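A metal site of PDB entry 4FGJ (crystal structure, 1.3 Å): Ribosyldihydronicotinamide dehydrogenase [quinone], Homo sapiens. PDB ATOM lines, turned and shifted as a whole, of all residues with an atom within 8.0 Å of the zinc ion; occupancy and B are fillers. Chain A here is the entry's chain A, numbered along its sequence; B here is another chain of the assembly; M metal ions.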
ATOM      1  N   TYR A 135      22.077 -22.522 -10.474  1.00  0.00           N
ATOM      2  CA  TYR A 135      22.064 -21.461  -9.480  1.00  0.00           C
ATOM      3  C   TYR A 135      23.497 -20.921  -9.298  1.00  0.00           C
ATOM      4  O   TYR A 135      24.103 -20.534 -10.298  1.00  0.00           O
ATOM      5  CB  TYR A 135      21.346 -21.922  -8.200  1.00  0.00           C
ATOM      6  CG  TYR A 135      19.834 -21.977  -8.420  1.00  0.00           C
ATOM      7  CD1 TYR A 135      19.138 -20.879  -8.932  1.00  0.00           C
ATOM      8  CD2 TYR A 135      19.102 -23.131  -8.160  1.00  0.00           C
ATOM      9  CE1 TYR A 135      17.761 -20.921  -9.148  1.00  0.00           C
ATOM     10  CE2 TYR A 135      17.720 -23.183  -8.357  1.00  0.00           C
ATOM     11  CZ  TYR A 135      17.063 -22.072  -8.862  1.00  0.00           C
ATOM     12  OH  TYR A 135      15.713 -22.083  -9.086  1.00  0.00           O
ATOM     13  N   ASP A 136      24.067 -20.905  -8.094  1.00  0.00           N
ATOM     14  CA  ASP A 136      25.373 -20.246  -7.935  1.00  0.00           C
ATOM     15  C   ASP A 136      26.470 -20.841  -8.815  1.00  0.00           C
ATOM     16  O   ASP A 136      27.435 -20.139  -9.196  1.00  0.00           O
ATOM     17  CB  ASP A 136      25.832 -20.271  -6.477  1.00  0.00           C
ATOM     18  CG  ASP A 136      25.057 -19.292  -5.616  1.00  0.00           C
ATOM     19  OD1 ASP A 136      24.214 -18.557  -6.171  1.00  0.00           O
ATOM     20  OD2 ASP A 136      25.312 -19.252  -4.395  1.00  0.00           O
ATOM     21  N   TRP A 172      10.619 -12.845 -10.457  1.00  0.00           N
ATOM     22  CA  TRP A 172      11.095 -14.138  -9.979  1.00  0.00           C
ATOM     23  C   TRP A 172      11.419 -15.149 -11.090  1.00  0.00           C
ATOM     24  O   TRP A 172      12.513 -15.706 -11.103  1.00  0.00           O
ATOM     25  CB  TRP A 172      10.104 -14.685  -8.953  1.00  0.00           C
ATOM     26  CG  TRP A 172      10.345 -16.036  -8.421  1.00  0.00           C
ATOM     27  CD1 TRP A 172       9.619 -17.165  -8.701  1.00  0.00           C
ATOM     28  CD2 TRP A 172      11.326 -16.420  -7.466  1.00  0.00           C
ATOM     29  NE1 TRP A 172      10.091 -18.222  -7.976  1.00  0.00           N
ATOM     30  CE2 TRP A 172      11.143 -17.791  -7.207  1.00  0.00           C
ATOM     31  CE3 TRP A 172      12.353 -15.735  -6.794  1.00  0.00           C
ATOM     32  CZ2 TRP A 172      11.953 -18.501  -6.316  1.00  0.00           C
ATOM     33  CZ3 TRP A 172      13.149 -16.441  -5.910  1.00  0.00           C
ATOM     34  CH2 TRP A 172      12.925 -17.807  -5.675  1.00  0.00           C
ATOM     35  N   LEU A 174      12.124 -14.718 -14.145  1.00  0.00           N
ATOM     36  CA  LEU A 174      13.188 -14.203 -15.013  1.00  0.00           C
ATOM     37  C   LEU A 174      14.538 -14.138 -14.297  1.00  0.00           C
ATOM     38  O   LEU A 174      15.528 -14.717 -14.760  1.00  0.00           O
ATOM     39  CB  LEU A 174      12.783 -12.819 -15.516  1.00  0.00           C
ATOM     40  CG  LEU A 174      11.502 -12.794 -16.358  1.00  0.00           C
ATOM     41  CD1 LEU A 174      11.053 -11.372 -16.654  1.00  0.00           C
ATOM     42  CD2 LEU A 174      11.696 -13.577 -17.637  1.00  0.00           C
ATOM     43  N   GLN A 175      14.582 -13.430 -13.167  1.00  0.00           N
ATOM     44  CA  GLN A 175      15.828 -13.242 -12.436  1.00  0.00           C
ATOM     45  C   GLN A 175      16.282 -14.512 -11.777  1.00  0.00           C
ATOM     46  O   GLN A 175      17.450 -14.875 -11.878  1.00  0.00           O
ATOM     47  CB  GLN A 175      15.679 -12.135 -11.394  1.00  0.00           C
ATOM     48  CG  GLN A 175      15.460 -10.785 -12.011  1.00  0.00           C
ATOM     49  CD  GLN A 175      15.565  -9.630 -11.036  1.00  0.00           C
ATOM     50  OE1 GLN A 175      15.876  -8.514 -11.449  1.00  0.00           O
ATOM     51  NE2 GLN A 175      15.278  -9.872  -9.758  1.00  0.00           N
ATOM     52  N   HIS A 176      15.364 -15.202 -11.093  1.00  0.00           N
ATOM     53  CA  HIS A 176      15.764 -16.367 -10.316  1.00  0.00           C
ATOM     54  C   HIS A 176      15.668 -17.639 -11.148  1.00  0.00           C
ATOM     55  O   HIS A 176      16.638 -18.377 -11.287  1.00  0.00           O
ATOM     56  CB  HIS A 176      14.935 -16.495  -9.045  1.00  0.00           C
ATOM     57  CG  HIS A 176      15.357 -17.635  -8.174  1.00  0.00           C
ATOM     58  ND1 HIS A 176      16.506 -17.590  -7.414  1.00  0.00           N
ATOM     59  CD2 HIS A 176      14.805 -18.846  -7.949  1.00  0.00           C
ATOM     60  CE1 HIS A 176      16.649 -18.731  -6.761  1.00  0.00           C
ATOM     61  NE2 HIS A 176      15.618 -19.505  -7.059  1.00  0.00           N
ATOM     62  N   GLY A 177      14.474 -17.901 -11.704  1.00  0.00           N
ATOM     63  CA  GLY A 177      14.244 -19.129 -12.427  1.00  0.00           C
ATOM     64  C   GLY A 177      15.060 -19.291 -13.695  1.00  0.00           C
ATOM     65  O   GLY A 177      15.292 -20.411 -14.157  1.00  0.00           O
ATOM     66  N   THR A 178      15.477 -18.161 -14.274  1.00  0.00           N
ATOM     67  CA  THR A 178      16.246 -18.177 -15.520  1.00  0.00           C
ATOM     68  C   THR A 178      17.687 -17.686 -15.318  1.00  0.00           C
ATOM     69  O   THR A 178      18.620 -18.475 -15.399  1.00  0.00           O
ATOM     70  CB  THR A 178      15.523 -17.353 -16.630  1.00  0.00           C
ATOM     71  OG1 THR A 178      14.138 -17.745 -16.741  1.00  0.00           O
ATOM     72  CG2 THR A 178      16.204 -17.550 -17.957  1.00  0.00           C
ATOM     73  N   LEU A 179      17.857 -16.418 -14.988  1.00  0.00           N
ATOM     74  CA  LEU A 179      19.214 -15.842 -14.943  1.00  0.00           C
ATOM     75  C   LEU A 179      20.074 -16.436 -13.813  1.00  0.00           C
ATOM     76  O   LEU A 179      21.190 -16.907 -14.050  1.00  0.00           O
ATOM     77  CB  LEU A 179      19.129 -14.322 -14.853  1.00  0.00           C
ATOM     78  CG  LEU A 179      18.440 -13.661 -16.046  1.00  0.00           C
ATOM     79  CD1 LEU A 179      18.302 -12.182 -15.791  1.00  0.00           C
ATOM     80  CD2 LEU A 179      19.147 -13.952 -17.372  1.00  0.00           C
ATOM     81  N   HIS A 180      19.572 -16.426 -12.585  1.00  0.00           N
ATOM     82  CA  HIS A 180      20.321 -17.015 -11.469  1.00  0.00           C
ATOM     83  C   HIS A 180      20.530 -18.494 -11.734  1.00  0.00           C
ATOM     84  O   HIS A 180      21.592 -19.044 -11.433  1.00  0.00           O
ATOM     85  CB  HIS A 180      19.565 -16.797 -10.169  1.00  0.00           C
ATOM     86  CG  HIS A 180      20.310 -17.211  -8.941  1.00  0.00           C
ATOM     87  ND1 HIS A 180      19.778 -17.045  -7.681  1.00  0.00           N
ATOM     88  CD2 HIS A 180      21.546 -17.740  -8.753  1.00  0.00           C
ATOM     89  CE1 HIS A 180      20.623 -17.479  -6.777  1.00  0.00           C
ATOM     90  NE2 HIS A 180      21.703 -17.909  -7.401  1.00  0.00           N
ATOM     91  N   PHE A 181      19.514 -19.172 -12.264  1.00  0.00           N
ATOM     92  CA  PHE A 181      19.642 -20.599 -12.508  1.00  0.00           C
ATOM     93  C   PHE A 181      20.861 -20.887 -13.372  1.00  0.00           C
ATOM     94  O   PHE A 181      21.573 -21.855 -13.137  1.00  0.00           O
ATOM     95  CB  PHE A 181      18.365 -21.174 -13.148  1.00  0.00           C
ATOM     96  CG  PHE A 181      18.363 -22.671 -13.212  1.00  0.00           C
ATOM     97  CD1 PHE A 181      18.067 -23.417 -12.082  1.00  0.00           C
ATOM     98  CD2 PHE A 181      18.649 -23.335 -14.391  1.00  0.00           C
ATOM     99  CE1 PHE A 181      18.061 -24.796 -12.146  1.00  0.00           C
ATOM    100  CE2 PHE A 181      18.646 -24.701 -14.453  1.00  0.00           C
ATOM    101  CZ  PHE A 181      18.351 -25.431 -13.330  1.00  0.00           C
ATOM    102  N   PHE A 184      24.235 -16.501 -13.654  1.00  0.00           N
ATOM    103  CA  PHE A 184      24.443 -15.068 -13.670  1.00  0.00           C
ATOM    104  C   PHE A 184      24.348 -14.503 -12.248  1.00  0.00           C
ATOM    105  O   PHE A 184      23.515 -14.953 -11.432  1.00  0.00           O
ATOM    106  CB  PHE A 184      23.375 -14.345 -14.503  1.00  0.00           C
ATOM    107  CG  PHE A 184      23.494 -14.511 -15.992  1.00  0.00           C
ATOM    108  CD1 PHE A 184      24.389 -13.751 -16.722  1.00  0.00           C
ATOM    109  CD2 PHE A 184      22.643 -15.356 -16.687  1.00  0.00           C
ATOM    110  CE1 PHE A 184      24.467 -13.850 -18.102  1.00  0.00           C
ATOM    111  CE2 PHE A 184      22.715 -15.465 -18.088  1.00  0.00           C
ATOM    112  CZ  PHE A 184      23.631 -14.699 -18.789  1.00  0.00           C
ATOM    113  N   VAL A 186      22.887 -11.232 -10.792  1.00  0.00           N
ATOM    114  CA  VAL A 186      21.834 -10.411 -11.313  1.00  0.00           C
ATOM    115  C   VAL A 186      21.973  -9.015 -10.753  1.00  0.00           C
ATOM    116  O   VAL A 186      21.910  -8.799  -9.549  1.00  0.00           O
ATOM    117  CB  VAL A 186      20.482 -10.996 -10.889  1.00  0.00           C
ATOM    118  CG1 VAL A 186      19.330 -10.113 -11.334  1.00  0.00           C
ATOM    119  CG2 VAL A 186      20.339 -12.389 -11.469  1.00  0.00           C
ATOM    120  N   ILE A 223      22.244  -8.036  -6.800  1.00  0.00           N
ATOM    121  CA  ILE A 223      21.264  -8.288  -5.755  1.00  0.00           C
ATOM    122  C   ILE A 223      21.442  -9.688  -5.192  1.00  0.00           C
ATOM    123  O   ILE A 223      22.014 -10.550  -5.841  1.00  0.00           O
ATOM    124  CB  ILE A 223      19.801  -8.174  -6.270  1.00  0.00           C
ATOM    125  CG1 ILE A 223      19.507  -9.263  -7.309  1.00  0.00           C
ATOM    126  CG2 ILE A 223      19.533  -6.784  -6.832  1.00  0.00           C
ATOM    127  CD1 ILE A 223      18.024  -9.404  -7.691  1.00  0.00           C
ATOM    128  N   PRO A 224      20.959  -9.909  -3.965  1.00  0.00           N
ATOM    129  CA  PRO A 224      20.862 -11.274  -3.471  1.00  0.00           C
ATOM    130  C   PRO A 224      19.617 -11.900  -4.114  1.00  0.00           C
ATOM    131  O   PRO A 224      18.494 -11.540  -3.753  1.00  0.00           O
ATOM    132  CB  PRO A 224      20.703 -11.102  -1.965  1.00  0.00           C
ATOM    133  CG  PRO A 224      20.022  -9.765  -1.813  1.00  0.00           C
ATOM    134  CD  PRO A 224      20.435  -8.926  -3.006  1.00  0.00           C
ATOM    135  N   CYS A 225      19.823 -12.780  -5.084  1.00  0.00           N
ATOM    136  CA  CYS A 225      18.711 -13.304  -5.881  1.00  0.00           C
ATOM    137  C   CYS A 225      18.046 -14.468  -5.140  1.00  0.00           C
ATOM    138  O   CYS A 225      18.242 -15.637  -5.452  1.00  0.00           O
ATOM    139  CB  CYS A 225      19.183 -13.731  -7.270  1.00  0.00           C
ATOM    140  SG  CYS A 225      17.785 -14.121  -8.353  1.00  0.00           S
ATOM    141  N   THR A 226      17.282 -14.085  -4.118  1.00  0.00           N
ATOM    142  CA  THR A 226      16.673 -15.037  -3.205  1.00  0.00           C
ATOM    143  C   THR A 226      15.166 -14.834  -3.145  1.00  0.00           C
ATOM    144  O   THR A 226      14.649 -13.785  -3.537  1.00  0.00           O
ATOM    145  CB  THR A 226      17.222 -14.798  -1.785  1.00  0.00           C
ATOM    146  OG1 THR A 226      16.838 -13.484  -1.371  1.00  0.00           O
ATOM    147  CG2 THR A 226      18.724 -14.918  -1.758  1.00  0.00           C
ATOM    148  N   ALA A 227      14.464 -15.822  -2.605  1.00  0.00           N
ATOM    149  CA  ALA A 227      13.026 -15.700  -2.394  1.00  0.00           C
ATOM    150  C   ALA A 227      12.750 -14.512  -1.464  1.00  0.00           C
ATOM    151  O   ALA A 227      11.811 -13.745  -1.682  1.00  0.00           O
ATOM    152  CB  ALA A 227      12.445 -16.999  -1.812  1.00  0.00           C
ATOM    153  N   TRP A 229      14.417 -11.717  -1.159  1.00  0.00           N
ATOM    154  CA  TRP A 229      14.543 -10.457  -1.880  1.00  0.00           C
ATOM    155  C   TRP A 229      13.274 -10.213  -2.687  1.00  0.00           C
ATOM    156  O   TRP A 229      12.763  -9.088  -2.749  1.00  0.00           O
ATOM    157  CB  TRP A 229      15.752 -10.477  -2.810  1.00  0.00           C
ATOM    158  CG  TRP A 229      16.016  -9.172  -3.501  1.00  0.00           C
ATOM    159  CD1 TRP A 229      16.856  -8.175  -3.086  1.00  0.00           C
ATOM    160  CD2 TRP A 229      15.458  -8.715  -4.758  1.00  0.00           C
ATOM    161  NE1 TRP A 229      16.848  -7.139  -3.981  1.00  0.00           N
ATOM    162  CE2 TRP A 229      16.007  -7.447  -5.024  1.00  0.00           C
ATOM    163  CE3 TRP A 229      14.549  -9.261  -5.669  1.00  0.00           C
ATOM    164  CZ2 TRP A 229      15.670  -6.701  -6.139  1.00  0.00           C
ATOM    165  CZ3 TRP A 229      14.222  -8.514  -6.805  1.00  0.00           C
ATOM    166  CH2 TRP A 229      14.786  -7.247  -7.033  1.00  0.00           C
ATOM    167  N   HIS A 230      12.761 -11.261  -3.309  1.00  0.00           N
ATOM    168  CA  HIS A 230      11.612 -11.110  -4.210  1.00  0.00           C
ATOM    169  C   HIS A 230      10.283 -10.988  -3.451  1.00  0.00           C
ATOM    170  O   HIS A 230       9.410 -10.236  -3.866  1.00  0.00           O
ATOM    171  CB  HIS A 230      11.545 -12.286  -5.193  1.00  0.00           C
ATOM    172  CG  HIS A 230      12.611 -12.257  -6.247  1.00  0.00           C
ATOM    173  ND1 HIS A 230      13.872 -12.750  -6.046  1.00  0.00           N
ATOM    174  CD2 HIS A 230      12.574 -11.831  -7.541  1.00  0.00           C
ATOM    175  CE1 HIS A 230      14.586 -12.605  -7.155  1.00  0.00           C
ATOM    176  NE2 HIS A 230      13.820 -12.055  -8.070  1.00  0.00           N
ATOM    177  N   VAL B 163      15.117 -25.230  -3.516  1.00  0.00           N
ATOM    178  CA  VAL B 163      15.966 -24.348  -4.310  1.00  0.00           C
ATOM    179  C   VAL B 163      15.168 -23.496  -5.292  1.00  0.00           C
ATOM    180  O   VAL B 163      15.568 -22.368  -5.623  1.00  0.00           O
ATOM    181  CB  VAL B 163      17.038 -25.139  -5.108  1.00  0.00           C
ATOM    182  CG1 VAL B 163      18.088 -25.684  -4.160  1.00  0.00           C
ATOM    183  CG2 VAL B 163      16.392 -26.246  -5.927  1.00  0.00           C
HETATM  184 ZN    ZN M   1      17.960 -16.195  -7.415  1.00  0.00          ZN
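The side-chain hydroxyl of Thr 226 sits at hydrogen-bond distance from the backbone NH of Trp 229, at 3.0 Å. OD1 of Asp 136 is in hydrogen-bond range of NE2 of His 180. The backbone carbonyl oxygen of Gln 175 lies within hydrogen-bond range of the backbone NH of His 180 (2.7 Å). O of Thr 226 is in hydrogen-bond range of ND1 of His 230, 2.8 Å away. OG1 of Thr 226 lies within hydrogen-bond range of O of Pro 224, at 3.5 Å. A ring nitrogen (NE2) of His 176 sits at hydrogen-bond distance from the side-chain hydroxyl (OH) of Tyr 135, at 3.3 Å. N of Phe 181 sits at hydrogen-bond distance from O of His 176 (3.1 Å). The backbone carbonyl oxygen (O) of Gln 175 lies close to the side-chain sulfur (SG) of Cys 225, 3.6 Å away.
Merely in contact with the zinc ion: Thr 226. Of the 21 residues printed, 4 come within 4 Å of the zinc ion. The nearest printed residue that does not touch the zinc ion is Gln 175 (4.7 Å).
The zinc ion is bound by ND1 of His 176. ND1 of His 180 is bound to the zinc ion (2.0 Å). O of Cys 225 is bound to the zinc ion (2.1 Å). SG of Cys 225 is bound to the zinc ion. The zinc ion has four donor atoms within binding distance.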
